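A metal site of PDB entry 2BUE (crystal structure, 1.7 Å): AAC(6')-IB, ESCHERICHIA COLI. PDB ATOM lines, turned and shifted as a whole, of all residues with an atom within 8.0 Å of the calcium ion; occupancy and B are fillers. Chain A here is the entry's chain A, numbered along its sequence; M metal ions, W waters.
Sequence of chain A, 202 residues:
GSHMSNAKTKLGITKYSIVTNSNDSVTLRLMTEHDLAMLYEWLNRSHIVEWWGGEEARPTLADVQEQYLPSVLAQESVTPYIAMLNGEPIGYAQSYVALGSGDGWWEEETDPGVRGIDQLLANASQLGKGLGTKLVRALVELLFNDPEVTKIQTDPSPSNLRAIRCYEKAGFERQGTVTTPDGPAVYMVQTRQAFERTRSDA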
ATOM      1  N   GLN A 193     -27.110  -4.812   6.706  1.00  0.00           N
ATOM      2  CA  GLN A 193     -26.519  -4.532   8.033  1.00  0.00           C
ATOM      3  C   GLN A 193     -25.097  -5.091   8.135  1.00  0.00           C
ATOM      4  O   GLN A 193     -24.189  -4.416   8.642  1.00  0.00           O
ATOM      5  CB  GLN A 193     -27.403  -5.070   9.160  1.00  0.00           C
ATOM      6  CG  GLN A 193     -26.913  -4.623  10.567  1.00  0.00           C
ATOM      7  CD  GLN A 193     -27.826  -5.071  11.713  1.00  0.00           C
ATOM      8  OE1 GLN A 193     -28.126  -6.276  11.871  1.00  0.00           O
ATOM      9  NE2 GLN A 193     -28.258  -4.103  12.552  1.00  0.00           N
ATOM     10  N   ALA A 194     -24.901  -6.309   7.623  1.00  0.00           N
ATOM     11  CA  ALA A 194     -23.555  -6.910   7.596  1.00  0.00           C
ATOM     12  C   ALA A 194     -22.580  -6.091   6.782  1.00  0.00           C
ATOM     13  O   ALA A 194     -21.438  -5.878   7.209  1.00  0.00           O
ATOM     14  CB  ALA A 194     -23.622  -8.370   7.076  1.00  0.00           C
ATOM     15  N   PHE A 195     -23.024  -5.637   5.599  1.00  0.00           N
ATOM     16  CA  PHE A 195     -22.209  -4.830   4.701  1.00  0.00           C
ATOM     17  C   PHE A 195     -21.783  -3.527   5.397  1.00  0.00           C
ATOM     18  O   PHE A 195     -20.609  -3.121   5.322  1.00  0.00           O
ATOM     19  CB  PHE A 195     -22.997  -4.544   3.411  1.00  0.00           C
ATOM     20  CG  PHE A 195     -22.260  -3.703   2.425  1.00  0.00           C
ATOM     21  CD1 PHE A 195     -21.304  -4.270   1.593  1.00  0.00           C
ATOM     22  CD2 PHE A 195     -22.532  -2.323   2.339  1.00  0.00           C
ATOM     23  CE1 PHE A 195     -20.617  -3.479   0.648  1.00  0.00           C
ATOM     24  CE2 PHE A 195     -21.858  -1.529   1.412  1.00  0.00           C
ATOM     25  CZ  PHE A 195     -20.897  -2.100   0.567  1.00  0.00           C
ATOM     26  N   GLU A 196     -22.732  -2.877   6.062  1.00  0.00           N
ATOM     27  CA  GLU A 196     -22.473  -1.649   6.829  1.00  0.00           C
ATOM     28  C   GLU A 196     -21.423  -1.887   7.921  1.00  0.00           C
ATOM     29  O   GLU A 196     -20.436  -1.162   8.007  1.00  0.00           O
ATOM     30  CB  GLU A 196     -23.760  -1.128   7.473  1.00  0.00           C
ATOM     31  CG  GLU A 196     -24.785  -0.561   6.468  1.00  0.00           C
ATOM     32  CD  GLU A 196     -26.158  -0.358   7.085  1.00  0.00           C
ATOM     33  OE1 GLU A 196     -26.359  -0.697   8.272  1.00  0.00           O
ATOM     34  OE2 GLU A 196     -27.046   0.130   6.383  1.00  0.00           O
ATOM     35  N   ARG A 197     -21.637  -2.941   8.715  1.00  0.00           N
ATOM     36  CA  ARG A 197     -20.742  -3.268   9.832  1.00  0.00           C
ATOM     37  C   ARG A 197     -19.326  -3.536   9.375  1.00  0.00           C
ATOM     38  O   ARG A 197     -18.359  -3.172  10.076  1.00  0.00           O
ATOM     39  CB  ARG A 197     -21.278  -4.444  10.634  1.00  0.00           C
ATOM     40  CG  ARG A 197     -22.490  -4.124  11.471  1.00  0.00           C
ATOM     41  CD  ARG A 197     -22.903  -5.334  12.315  1.00  0.00           C
ATOM     42  NE  ARG A 197     -23.988  -6.151  11.737  1.00  0.00           N
ATOM     43  CZ  ARG A 197     -23.834  -7.366  11.191  1.00  0.00           C
ATOM     44  NH1 ARG A 197     -22.638  -7.931  11.096  1.00  0.00           N
ATOM     45  NH2 ARG A 197     -24.891  -8.008  10.718  1.00  0.00           N
ATOM     46  N   THR A 198     -19.178  -4.130   8.190  1.00  0.00           N
ATOM     47  CA  THR A 198     -17.857  -4.531   7.708  1.00  0.00           C
ATOM     48  C   THR A 198     -17.145  -3.484   6.870  1.00  0.00           C
ATOM     49  O   THR A 198     -16.034  -3.738   6.390  1.00  0.00           O
ATOM     50  CB  THR A 198     -17.876  -5.888   6.976  1.00  0.00           C
ATOM     51  OG1 THR A 198     -18.767  -5.809   5.849  1.00  0.00           O
ATOM     52  CG2 THR A 198     -18.345  -7.002   7.936  1.00  0.00           C
ATOM     53  N   ARG A 199     -17.741  -2.301   6.699  1.00  0.00           N
ATOM     54  CA  ARG A 199     -17.054  -1.236   5.925  1.00  0.00           C
ATOM     55  C   ARG A 199     -15.859  -0.622   6.656  1.00  0.00           C
ATOM     56  O   ARG A 199     -14.952  -0.095   6.019  1.00  0.00           O
ATOM     57  CB  ARG A 199     -18.000  -0.097   5.510  1.00  0.00           C
ATOM     58  CG  ARG A 199     -19.014  -0.438   4.425  1.00  0.00           C
ATOM     59  CD  ARG A 199     -18.468  -1.244   3.282  1.00  0.00           C
ATOM     60  NE  ARG A 199     -18.478  -2.681   3.594  1.00  0.00           N
ATOM     61  CZ  ARG A 199     -17.942  -3.624   2.844  1.00  0.00           C
ATOM     62  NH1 ARG A 199     -18.012  -4.890   3.228  1.00  0.00           N
ATOM     63  NH2 ARG A 199     -17.343  -3.310   1.696  1.00  0.00           N
ATOM     64  N   SER A 200     -15.892  -0.632   7.979  1.00  0.00           N
ATOM     65  CA  SER A 200     -14.757  -0.174   8.760  1.00  0.00           C
ATOM     66  C   SER A 200     -14.582  -0.996  10.030  1.00  0.00           C
ATOM     67  O   SER A 200     -15.536  -1.587  10.540  1.00  0.00           O
ATOM     68  CB  SER A 200     -14.866   1.325   9.082  1.00  0.00           C
ATOM     69  OG  SER A 200     -15.643   1.553  10.249  1.00  0.00           O
ATOM     70  N   ASP A 201     -13.344  -1.014  10.533  1.00  0.00           N
ATOM     71  CA  ASP A 201     -13.045  -1.702  11.777  1.00  0.00           C
ATOM     72  C   ASP A 201     -13.451  -0.879  13.010  1.00  0.00           C
ATOM     73  O   ASP A 201     -13.278  -1.300  14.156  1.00  0.00           O
ATOM     74  CB  ASP A 201     -11.554  -2.103  11.825  1.00  0.00           C
ATOM     75  CG  ASP A 201     -11.201  -3.161  10.775  1.00  0.00           C
ATOM     76  OD1 ASP A 201     -12.017  -4.090  10.537  1.00  0.00           O
ATOM     77  OD2 ASP A 201     -10.106  -3.066  10.172  1.00  0.00           O
ATOM     78  N   ALA A 202     -14.003   0.309  12.754  1.00  0.00           N
ATOM     79  CA  ALA A 202     -14.640   1.102  13.794  1.00  0.00           C
ATOM     80  C   ALA A 202     -16.022   0.529  14.169  1.00  0.00           C
ATOM     81  O   ALA A 202     -16.586  -0.381  13.516  1.00  0.00           O
ATOM     82  CB  ALA A 202     -14.746   2.567  13.365  1.00  0.00           C
ATOM     83  OXT ALA A 202     -16.626   0.929  15.163  1.00  0.00           O
HETATM   84 CA    CA M   1     -17.540  -1.917  11.889  1.00  0.00          CA
HETATM   85  O   HOH W   1     -16.410  -3.883  12.348  1.00  0.00           O
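N of Ala 202 sits close to OG of Ser 200, at 3.2 Å.
Three residues have an atom within 4 Å of the calcium ion: Arg 197, Ser 200 and Ala 202.
The calcium ion is bound by water W1, 2.3 Å away. The backbone carbonyl oxygen (O) of Arg 197 is bound to the calcium ion. The calcium ion is bound by O of Ala 202 (2.4 Å). The calcium ion is bound by O of Ser 200 (2.4 Å).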
